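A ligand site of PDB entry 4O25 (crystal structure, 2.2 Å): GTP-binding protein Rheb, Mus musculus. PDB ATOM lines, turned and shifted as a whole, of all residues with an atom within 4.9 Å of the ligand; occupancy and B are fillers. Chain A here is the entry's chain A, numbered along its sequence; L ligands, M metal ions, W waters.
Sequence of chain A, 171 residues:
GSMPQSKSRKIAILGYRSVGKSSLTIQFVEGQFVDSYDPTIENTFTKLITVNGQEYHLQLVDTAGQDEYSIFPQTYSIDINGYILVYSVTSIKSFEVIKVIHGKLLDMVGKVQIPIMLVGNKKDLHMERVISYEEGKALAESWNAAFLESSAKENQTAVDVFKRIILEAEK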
ATOM      1  N   TYR A  16       5.001  -3.853  -0.463  1.00  0.00           N
ATOM      2  CA  TYR A  16       5.565  -2.579  -0.923  1.00  0.00           C
ATOM      3  C   TYR A  16       7.039  -2.734  -1.248  1.00  0.00           C
ATOM      4  O   TYR A  16       7.696  -3.650  -0.768  1.00  0.00           O
ATOM      5  CB  TYR A  16       5.368  -1.513   0.160  1.00  0.00           C
ATOM      6  CG  TYR A  16       5.753  -0.102  -0.219  1.00  0.00           C
ATOM      7  CD1 TYR A  16       5.107   0.568  -1.248  1.00  0.00           C
ATOM      8  CD2 TYR A  16       6.740   0.573   0.485  1.00  0.00           C
ATOM      9  CE1 TYR A  16       5.451   1.882  -1.583  1.00  0.00           C
ATOM     10  CE2 TYR A  16       7.087   1.892   0.167  1.00  0.00           C
ATOM     11  CZ  TYR A  16       6.448   2.535  -0.856  1.00  0.00           C
ATOM     12  OH  TYR A  16       6.809   3.827  -1.175  1.00  0.00           O
ATOM     13  N   ARG A  17       7.568  -1.846  -2.070  1.00  0.00           N
ATOM     14  CA  ARG A  17       8.954  -1.988  -2.486  1.00  0.00           C
ATOM     15  C   ARG A  17       9.893  -1.816  -1.300  1.00  0.00           C
ATOM     16  O   ARG A  17       9.593  -1.047  -0.358  1.00  0.00           O
ATOM     17  CB  ARG A  17       9.298  -1.021  -3.645  1.00  0.00           C
ATOM     18  CG  ARG A  17       9.135   0.434  -3.308  1.00  0.00           C
ATOM     19  CD  ARG A  17       9.077   1.301  -4.580  1.00  0.00           C
ATOM     20  NE  ARG A  17       8.399   2.574  -4.322  1.00  0.00           N
ATOM     21  CZ  ARG A  17       7.125   2.830  -4.635  1.00  0.00           C
ATOM     22  NH1 ARG A  17       6.390   1.907  -5.248  1.00  0.00           N
ATOM     23  NH2 ARG A  17       6.593   4.013  -4.354  1.00  0.00           N
ATOM     24  N   SER A  18      10.977  -2.576  -1.324  1.00  0.00           N
ATOM     25  CA  SER A  18      12.081  -2.430  -0.391  1.00  0.00           C
ATOM     26  C   SER A  18      11.724  -2.975   0.992  1.00  0.00           C
ATOM     27  O   SER A  18      12.437  -2.714   1.965  1.00  0.00           O
ATOM     28  CB  SER A  18      12.529  -0.957  -0.316  1.00  0.00           C
ATOM     29  OG  SER A  18      13.909  -0.844  -0.033  1.00  0.00           O
ATOM     30  N   VAL A  19      10.648  -3.739   1.090  1.00  0.00           N
ATOM     31  CA  VAL A  19      10.285  -4.318   2.374  1.00  0.00           C
ATOM     32  C   VAL A  19      11.090  -5.580   2.695  1.00  0.00           C
ATOM     33  O   VAL A  19      11.076  -6.040   3.834  1.00  0.00           O
ATOM     34  CB  VAL A  19       8.774  -4.643   2.472  1.00  0.00           C
ATOM     35  CG1 VAL A  19       7.940  -3.364   2.312  1.00  0.00           C
ATOM     36  CG2 VAL A  19       8.396  -5.717   1.468  1.00  0.00           C
ATOM     37  N   GLY A  20      11.769  -6.120   1.685  1.00  0.00           N
ATOM     38  CA  GLY A  20      12.562  -7.327   1.875  1.00  0.00           C
ATOM     39  C   GLY A  20      11.928  -8.600   1.354  1.00  0.00           C
ATOM     40  O   GLY A  20      12.257  -9.678   1.840  1.00  0.00           O
ATOM     41  N   LYS A  21      11.045  -8.493   0.347  1.00  0.00           N
ATOM     42  CA  LYS A  21      10.444  -9.665  -0.292  1.00  0.00           C
ATOM     43  C   LYS A  21      11.535 -10.528  -0.895  1.00  0.00           C
ATOM     44  O   LYS A  21      11.589 -11.734  -0.651  1.00  0.00           O
ATOM     45  CB  LYS A  21       9.462  -9.276  -1.388  1.00  0.00           C
ATOM     46  CG  LYS A  21       8.219  -8.535  -0.931  1.00  0.00           C
ATOM     47  CD  LYS A  21       7.275  -8.255  -2.112  1.00  0.00           C
ATOM     48  CE  LYS A  21       7.898  -7.347  -3.144  1.00  0.00           C
ATOM     49  NZ  LYS A  21       8.202  -6.008  -2.568  1.00  0.00           N
ATOM     50  N   SER A  22      12.416  -9.909  -1.671  1.00  0.00           N
ATOM     51  CA  SER A  22      13.518 -10.639  -2.293  1.00  0.00           C
ATOM     52  C   SER A  22      14.548 -11.150  -1.287  1.00  0.00           C
ATOM     53  O   SER A  22      14.974 -12.308  -1.381  1.00  0.00           O
ATOM     54  CB  SER A  22      14.195  -9.799  -3.383  1.00  0.00           C
ATOM     55  OG  SER A  22      13.247  -9.415  -4.356  1.00  0.00           O
ATOM     56  N   SER A  23      14.933 -10.319  -0.328  1.00  0.00           N
ATOM     57  CA  SER A  23      15.892 -10.737   0.708  1.00  0.00           C
ATOM     58  C   SER A  23      15.409 -11.947   1.520  1.00  0.00           C
ATOM     59  O   SER A  23      16.181 -12.870   1.782  1.00  0.00           O
ATOM     60  CB  SER A  23      16.222  -9.588   1.669  1.00  0.00           C
ATOM     61  OG  SER A  23      17.030  -8.618   1.053  1.00  0.00           O
ATOM     62  N   PHE A  33      22.231 -13.538   2.750  1.00  0.00           N
ATOM     63  CA  PHE A  33      21.608 -12.223   2.843  1.00  0.00           C
ATOM     64  C   PHE A  33      22.221 -11.261   1.827  1.00  0.00           C
ATOM     65  O   PHE A  33      23.444 -11.120   1.759  1.00  0.00           O
ATOM     66  CB  PHE A  33      21.712 -11.667   4.276  1.00  0.00           C
ATOM     67  CG  PHE A  33      21.135 -10.295   4.422  1.00  0.00           C
ATOM     68  CD1 PHE A  33      19.777 -10.086   4.289  1.00  0.00           C
ATOM     69  CD2 PHE A  33      21.958  -9.201   4.658  1.00  0.00           C
ATOM     70  CE1 PHE A  33      19.238  -8.818   4.403  1.00  0.00           C
ATOM     71  CE2 PHE A  33      21.429  -7.932   4.794  1.00  0.00           C
ATOM     72  CZ  PHE A  33      20.065  -7.741   4.655  1.00  0.00           C
ATOM     73  N   VAL A  34      21.380 -10.607   1.040  1.00  0.00           N
ATOM     74  CA  VAL A  34      21.845  -9.647   0.056  1.00  0.00           C
ATOM     75  C   VAL A  34      21.513  -8.220   0.497  1.00  0.00           C
ATOM     76  O   VAL A  34      20.615  -8.001   1.330  1.00  0.00           O
ATOM     77  CB  VAL A  34      21.226  -9.898  -1.315  1.00  0.00           C
ATOM     78  CG1 VAL A  34      21.495 -11.336  -1.758  1.00  0.00           C
ATOM     79  CG2 VAL A  34      19.734  -9.602  -1.286  1.00  0.00           C
ATOM     80  N   ASP A  35      22.239  -7.254  -0.045  1.00  0.00           N
ATOM     81  CA  ASP A  35      21.978  -5.838   0.206  1.00  0.00           C
ATOM     82  C   ASP A  35      21.417  -5.172  -1.054  1.00  0.00           C
ATOM     83  O   ASP A  35      20.940  -4.039  -1.004  1.00  0.00           O
ATOM     84  CB  ASP A  35      23.260  -5.141   0.677  1.00  0.00           C
ATOM     85  CG  ASP A  35      24.075  -5.988   1.657  1.00  0.00           C
ATOM     86  OD1 ASP A  35      24.897  -6.812   1.202  1.00  0.00           O
ATOM     87  OD2 ASP A  35      23.905  -5.823   2.879  1.00  0.00           O
ATOM     88  N   SER A  36      21.465  -5.897  -2.179  1.00  0.00           N
ATOM     89  CA  SER A  36      21.003  -5.378  -3.471  1.00  0.00           C
ATOM     90  C   SER A  36      20.239  -6.433  -4.309  1.00  0.00           C
ATOM     91  O   SER A  36      20.223  -7.614  -3.953  1.00  0.00           O
ATOM     92  CB  SER A  36      22.166  -4.755  -4.264  1.00  0.00           C
ATOM     93  OG  SER A  36      21.705  -4.049  -5.410  1.00  0.00           O
ATOM     94  N   TYR A  37      19.626  -5.983  -5.413  1.00  0.00           N
ATOM     95  CA  TYR A  37      18.551  -6.713  -6.089  1.00  0.00           C
ATOM     96  C   TYR A  37      18.112  -6.024  -7.388  1.00  0.00           C
ATOM     97  O   TYR A  37      18.671  -4.985  -7.758  1.00  0.00           O
ATOM     98  CB  TYR A  37      17.339  -6.810  -5.157  1.00  0.00           C
ATOM     99  CG  TYR A  37      16.859  -5.459  -4.619  1.00  0.00           C
ATOM    100  CD1 TYR A  37      15.626  -4.936  -4.990  1.00  0.00           C
ATOM    101  CD2 TYR A  37      17.635  -4.716  -3.713  1.00  0.00           C
ATOM    102  CE1 TYR A  37      15.181  -3.696  -4.487  1.00  0.00           C
ATOM    103  CE2 TYR A  37      17.210  -3.481  -3.219  1.00  0.00           C
ATOM    104  CZ  TYR A  37      15.978  -2.976  -3.603  1.00  0.00           C
ATOM    105  OH  TYR A  37      15.553  -1.763  -3.108  1.00  0.00           O
ATOM    106  N   ASP A  38      17.117  -6.591  -8.074  1.00  0.00           N
ATOM    107  CA  ASP A  38      16.483  -5.933  -9.225  1.00  0.00           C
ATOM    108  C   ASP A  38      15.023  -5.620  -8.889  1.00  0.00           C
ATOM    109  O   ASP A  38      14.117  -6.362  -9.282  1.00  0.00           O
ATOM    110  CB  ASP A  38      16.533  -6.817 -10.480  1.00  0.00           C
ATOM    111  CG  ASP A  38      17.956  -7.138 -10.930  1.00  0.00           C
ATOM    112  OD1 ASP A  38      18.540  -6.364 -11.728  1.00  0.00           O
ATOM    113  OD2 ASP A  38      18.461  -8.202 -10.515  1.00  0.00           O
ATOM    114  N   PRO A  39      14.785  -4.502  -8.189  1.00  0.00           N
ATOM    115  CA  PRO A  39      13.506  -4.116  -7.574  1.00  0.00           C
ATOM    116  C   PRO A  39      12.241  -4.383  -8.394  1.00  0.00           C
ATOM    117  O   PRO A  39      11.313  -5.017  -7.873  1.00  0.00           O
ATOM    118  CB  PRO A  39      13.681  -2.603  -7.313  1.00  0.00           C
ATOM    119  CG  PRO A  39      14.965  -2.194  -8.010  1.00  0.00           C
ATOM    120  CD  PRO A  39      15.797  -3.437  -8.039  1.00  0.00           C
ATOM    121  N   THR A  40      12.184  -3.922  -9.635  1.00  0.00           N
ATOM    122  CA  THR A  40      10.935  -3.946 -10.403  1.00  0.00           C
ATOM    123  C   THR A  40      10.757  -5.183 -11.282  1.00  0.00           C
ATOM    124  O   THR A  40       9.989  -5.153 -12.239  1.00  0.00           O
ATOM    125  CB  THR A  40      10.749  -2.655 -11.285  1.00  0.00           C
ATOM    126  OG1 THR A  40      11.733  -2.600 -12.323  1.00  0.00           O
ATOM    127  CG2 THR A  40      10.835  -1.389 -10.432  1.00  0.00           C
ATOM    128  N   ASP A  62       8.548 -14.157  -6.538  1.00  0.00           N
ATOM    129  CA  ASP A  62       8.971 -12.926  -5.923  1.00  0.00           C
ATOM    130  C   ASP A  62       8.567 -11.789  -6.849  1.00  0.00           C
ATOM    131  O   ASP A  62       9.169 -11.575  -7.893  1.00  0.00           O
ATOM    132  CB  ASP A  62      10.480 -12.948  -5.712  1.00  0.00           C
ATOM    133  CG  ASP A  62      10.993 -11.714  -5.030  1.00  0.00           C
ATOM    134  OD1 ASP A  62      10.266 -11.178  -4.169  1.00  0.00           O
ATOM    135  OD2 ASP A  62      12.113 -11.268  -5.367  1.00  0.00           O
ATOM    136  N   THR A  63       7.504 -11.091  -6.459  1.00  0.00           N
ATOM    137  CA  THR A  63       6.828 -10.168  -7.344  1.00  0.00           C
ATOM    138  C   THR A  63       7.503  -8.800  -7.333  1.00  0.00           C
ATOM    139  O   THR A  63       8.211  -8.455  -6.379  1.00  0.00           O
ATOM    140  CB  THR A  63       5.344 -10.001  -6.934  1.00  0.00           C
ATOM    141  OG1 THR A  63       5.266  -9.380  -5.648  1.00  0.00           O
ATOM    142  CG2 THR A  63       4.635 -11.351  -6.894  1.00  0.00           C
ATOM    143  N   ALA A  64       7.288  -8.011  -8.383  1.00  0.00           N
ATOM    144  CA  ALA A  64       7.697  -6.616  -8.368  1.00  0.00           C
ATOM    145  C   ALA A  64       6.858  -5.889  -7.314  1.00  0.00           C
ATOM    146  O   ALA A  64       5.674  -6.167  -7.169  1.00  0.00           O
ATOM    147  CB  ALA A  64       7.486  -5.987  -9.733  1.00  0.00           C
ATOM    148  N   GLY A  65       7.457  -4.966  -6.581  1.00  0.00           N
ATOM    149  CA  GLY A  65       6.741  -4.343  -5.471  1.00  0.00           C
ATOM    150  C   GLY A  65       5.445  -3.652  -5.887  1.00  0.00           C
ATOM    151  O   GLY A  65       5.370  -3.067  -6.971  1.00  0.00           O
ATOM    152  N   ASN A 121       8.609  -7.760   8.287  1.00  0.00           N
ATOM    153  CA  ASN A 121      10.036  -8.024   8.121  1.00  0.00           C
ATOM    154  C   ASN A 121      10.925  -6.928   8.748  1.00  0.00           C
ATOM    155  O   ASN A 121      10.442  -5.862   9.140  1.00  0.00           O
ATOM    156  CB  ASN A 121      10.362  -8.194   6.623  1.00  0.00           C
ATOM    157  CG  ASN A 121      11.721  -8.811   6.387  1.00  0.00           C
ATOM    158  OD1 ASN A 121      12.110  -9.749   7.071  1.00  0.00           O
ATOM    159  ND2 ASN A 121      12.455  -8.280   5.416  1.00  0.00           N
ATOM    160  N   LYS A 122      12.237  -7.207   8.801  1.00  0.00           N
ATOM    161  CA  LYS A 122      13.258  -6.282   9.293  1.00  0.00           C
ATOM    162  C   LYS A 122      13.161  -6.050  10.793  1.00  0.00           C
ATOM    163  O   LYS A 122      13.489  -4.976  11.273  1.00  0.00           O
ATOM    164  CB  LYS A 122      13.245  -4.922   8.563  1.00  0.00           C
ATOM    165  CG  LYS A 122      13.225  -4.996   7.040  1.00  0.00           C
ATOM    166  CD  LYS A 122      13.496  -3.601   6.413  1.00  0.00           C
ATOM    167  CE  LYS A 122      13.626  -3.672   4.888  1.00  0.00           C
ATOM    168  NZ  LYS A 122      13.974  -2.339   4.264  1.00  0.00           N
ATOM    169  N   ASP A 124      15.030  -6.994  12.876  1.00  0.00           N
ATOM    170  CA  ASP A 124      16.371  -6.791  13.417  1.00  0.00           C
ATOM    171  C   ASP A 124      16.749  -5.322  13.551  1.00  0.00           C
ATOM    172  O   ASP A 124      17.665  -4.956  14.302  1.00  0.00           O
ATOM    173  CB  ASP A 124      17.422  -7.531  12.563  1.00  0.00           C
ATOM    174  CG  ASP A 124      17.446  -7.051  11.127  1.00  0.00           C
ATOM    175  OD1 ASP A 124      16.598  -7.516  10.330  1.00  0.00           O
ATOM    176  OD2 ASP A 124      18.322  -6.221  10.785  1.00  0.00           O
ATOM    177  N   LEU A 125      16.051  -4.449  12.821  1.00  0.00           N
ATOM    178  CA  LEU A 125      16.367  -3.037  12.887  1.00  0.00           C
ATOM    179  C   LEU A 125      15.657  -2.394  14.069  1.00  0.00           C
ATOM    180  O   LEU A 125      14.722  -1.614  13.890  1.00  0.00           O
ATOM    181  CB  LEU A 125      16.001  -2.346  11.572  1.00  0.00           C
ATOM    182  CG  LEU A 125      16.856  -2.874  10.423  1.00  0.00           C
ATOM    183  CD1 LEU A 125      16.547  -2.165   9.091  1.00  0.00           C
ATOM    184  CD2 LEU A 125      18.350  -2.762  10.794  1.00  0.00           C
ATOM    185  N   SER A 150       9.847 -11.209  10.861  1.00  0.00           N
ATOM    186  CA  SER A 150      11.012 -11.885  10.321  1.00  0.00           C
ATOM    187  C   SER A 150      12.194 -10.947  10.142  1.00  0.00           C
ATOM    188  O   SER A 150      12.049  -9.727  10.177  1.00  0.00           O
ATOM    189  CB  SER A 150      10.687 -12.560   8.988  1.00  0.00           C
ATOM    190  OG  SER A 150      10.346 -11.601   7.999  1.00  0.00           O
ATOM    191  N   SER A 151      13.370 -11.552   9.972  1.00  0.00           N
ATOM    192  CA  SER A 151      14.554 -10.839   9.516  1.00  0.00           C
ATOM    193  C   SER A 151      15.245 -11.654   8.452  1.00  0.00           C
ATOM    194  O   SER A 151      15.677 -12.780   8.723  1.00  0.00           O
ATOM    195  CB  SER A 151      15.569 -10.619  10.636  1.00  0.00           C
ATOM    196  OG  SER A 151      16.734 -10.007  10.098  1.00  0.00           O
ATOM    197  N   ALA A 152      15.362 -11.081   7.258  1.00  0.00           N
ATOM    198  CA  ALA A 152      16.030 -11.763   6.146  1.00  0.00           C
ATOM    199  C   ALA A 152      17.495 -12.078   6.467  1.00  0.00           C
ATOM    200  O   ALA A 152      18.140 -12.849   5.749  1.00  0.00           O
ATOM    201  CB  ALA A 152      15.942 -10.924   4.888  1.00  0.00           C
ATOM    202  N   LYS A 153      18.012 -11.456   7.531  1.00  0.00           N
ATOM    203  CA  LYS A 153      19.341 -11.773   8.053  1.00  0.00           C
ATOM    204  C   LYS A 153      19.364 -13.077   8.844  1.00  0.00           C
ATOM    205  O   LYS A 153      20.433 -13.637   9.125  1.00  0.00           O
ATOM    206  CB  LYS A 153      19.831 -10.645   8.968  1.00  0.00           C
ATOM    207  CG  LYS A 153      20.378  -9.450   8.240  1.00  0.00           C
ATOM    208  CD  LYS A 153      20.881  -8.428   9.234  1.00  0.00           C
ATOM    209  CE  LYS A 153      21.680  -7.361   8.530  1.00  0.00           C
ATOM    210  NZ  LYS A 153      21.956  -6.220   9.430  1.00  0.00           N
HETATM  211  P1  LIG L   1      11.299  -4.699  -4.381  1.00  0.00           P
HETATM  212  O1  LIG L   1      11.617  -3.348  -4.993  1.00  0.00           O
HETATM  213  O2  LIG L   1       9.789  -4.864  -4.339  1.00  0.00           O
HETATM  214  O3  LIG L   1      11.980  -5.806  -5.158  1.00  0.00           O
HETATM  215  O4  LIG L   1      11.866  -4.664  -2.855  1.00  0.00           O
HETATM  216  P2  LIG L   1      12.000  -5.982  -1.966  1.00  0.00           P
HETATM  217  O5  LIG L   1      12.436  -7.193  -2.771  1.00  0.00           O
HETATM  218  O6  LIG L   1      10.686  -6.216  -1.229  1.00  0.00           O
HETATM  219  O7  LIG L   1      13.124  -5.595  -0.870  1.00  0.00           O
HETATM  220  P3  LIG L   1      14.628  -6.168  -0.873  1.00  0.00           P
HETATM  221  O8  LIG L   1      15.346  -5.796  -2.136  1.00  0.00           O
HETATM  222  O9  LIG L   1      14.677  -7.654  -0.603  1.00  0.00           O
HETATM  223  O10 LIG L   1      15.265  -5.308   0.322  1.00  0.00           O
HETATM  224  C1  LIG L   1      15.326  -3.913   0.230  1.00  0.00           C
HETATM  225  C2  LIG L   1      16.505  -3.486   1.093  1.00  0.00           C
HETATM  226  O11 LIG L   1      16.218  -3.843   2.429  1.00  0.00           O
HETATM  227  C3  LIG L   1      17.786  -4.210   0.721  1.00  0.00           C
HETATM  228  O12 LIG L   1      18.823  -3.267   0.842  1.00  0.00           O
HETATM  229  C4  LIG L   1      17.936  -5.281   1.797  1.00  0.00           C
HETATM  230  O13 LIG L   1      19.281  -5.618   2.039  1.00  0.00           O
HETATM  231  C5  LIG L   1      17.256  -4.642   2.992  1.00  0.00           C
HETATM  232  N1  LIG L   1      16.614  -5.648   3.861  1.00  0.00           N
HETATM  233  C6  LIG L   1      15.633  -6.504   3.456  1.00  0.00           C
HETATM  234  N2  LIG L   1      15.264  -7.254   4.511  1.00  0.00           N
HETATM  235  C7  LIG L   1      15.982  -6.870   5.580  1.00  0.00           C
HETATM  236  C8  LIG L   1      15.993  -7.316   6.901  1.00  0.00           C
HETATM  237  O14 LIG L   1      15.228  -8.221   7.248  1.00  0.00           O
HETATM  238  N3  LIG L   1      16.849  -6.746   7.811  1.00  0.00           N
HETATM  239  C9  LIG L   1      17.688  -5.733   7.423  1.00  0.00           C
HETATM  240  N4  LIG L   1      18.512  -5.191   8.318  1.00  0.00           N
HETATM  241  N5  LIG L   1      17.681  -5.301   6.106  1.00  0.00           N
HETATM  242  C10 LIG L   1      16.837  -5.853   5.193  1.00  0.00           C
HETATM  243 MG    MG M   1      10.776  -8.312  -4.985  1.00  0.00          MG
HETATM  244  O   HOH W   1      13.034  -8.114  -6.595  1.00  0.00           O
HETATM  245  O   HOH W   2      13.014  -1.569  -3.897  1.00  0.00           O
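N of Lys 21 lies within hydrogen-bond range of O6 of the ligand. An oxygen (O2) of the ligand lies within salt-bridge range of the side-chain amino group of Lys 21. A nitrogen (N3) of the ligand lies within hydrogen-bond range of the side-chain carboxylate of Asp 124 (2.6 Å). N of Ser 23 sits at hydrogen-bond distance from O9 of the ligand, at 2.7 Å. The side-chain hydroxyl (OG) of Ser 23 lies within hydrogen-bond range of an oxygen (O9) of the ligand, at 3.0 Å. N of Ser 18 lies within hydrogen-bond range of O4 of the ligand, 2.7 Å away. An oxygen (O13) of the ligand sits at hydrogen-bond distance from the backbone carbonyl oxygen (O) of Val 34, 2.8 Å away. An oxygen (O5) of the ligand is in hydrogen-bond range of the backbone NH (N) of Ser 22 (2.9 Å). OG of Ser 22 is in hydrogen-bond range of O5 of the ligand. N of Ala 152 sits at hydrogen-bond distance from O14 of the ligand (2.9 Å). O3 of the ligand lies close to O of Pro 39 (2.9 Å). O of Asp 35 lies within hydrogen-bond range of O12 of the ligand (2.9 Å). N of Gly 20 lies within hydrogen-bond range of O7 of the ligand (2.9 Å). The side-chain amide nitrogen of Asn 121 sits at hydrogen-bond distance from a nitrogen (N2) of the ligand. The backbone NH (N) of Gly 65 is in hydrogen-bond range of an oxygen (O2) of the ligand, 3.2 Å away. An oxygen (O11) of the ligand sits at hydrogen-bond distance from the side-chain amino group of Lys 122 (3.3 Å). O6 of the ligand is in hydrogen-bond range of N of Val 19.
O of Tyr 16 lies within hydrogen-bond range of NZ of Lys 21 (3.0 Å). The side-chain hydroxyl (OG) of Ser 151 is in hydrogen-bond range of the side-chain carboxylate (OD1) of Asp 124, at 2.5 Å. The side-chain carboxylate (OD2) of Asp 124 lies within salt-bridge range of the side-chain amino group (NZ) of Lys 153, 3.9 Å away. The side-chain carboxylate (OD1) of Asp 62 lies close to the side-chain hydroxyl (OG) of Ser 22, 3.5 Å away. The side-chain amide nitrogen (ND2) of Asn 121 lies within hydrogen-bond range of the backbone carbonyl oxygen (O) of Val 19, 3.1 Å away. The side-chain amide oxygen (OD1) of Asn 121 sits at hydrogen-bond distance from the side-chain hydroxyl (OG) of Ser 150 (2.7 Å). The side-chain hydroxyl (OH) of Tyr 16 lies within hydrogen-bond range of the guanidinium group (NH2) of Arg 17. The backbone NH (N) of Lys 153 sits close to the side-chain hydroxyl (OG) of Ser 151 (3.2 Å).
Residues that only touch the ligand: Tyr 16, Arg 17, Phe 33, Tyr 37, Leu 125, Ser 151 and Lys 153. Hydrophobic or aromatic side chains within 4 Å of the ligand: Val 19, Phe 33, Tyr 37, Pro 39, Leu 125 and Ala 152.
Water W2 lies within hydrogen-bond range of an oxygen (O1) of the ligand (2.5 Å), the side-chain hydroxyl of Tyr 37 (2.7 Å) and the backbone NH of Ser 18 (3.4 Å). Water W1 lies within hydrogen-bond range of the side-chain hydroxyl (OG) of Ser 22 (2.6 Å), an oxygen (O3) of the ligand (2.9 Å) and the backbone carbonyl oxygen (O) of Asp 38 (3.4 Å).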
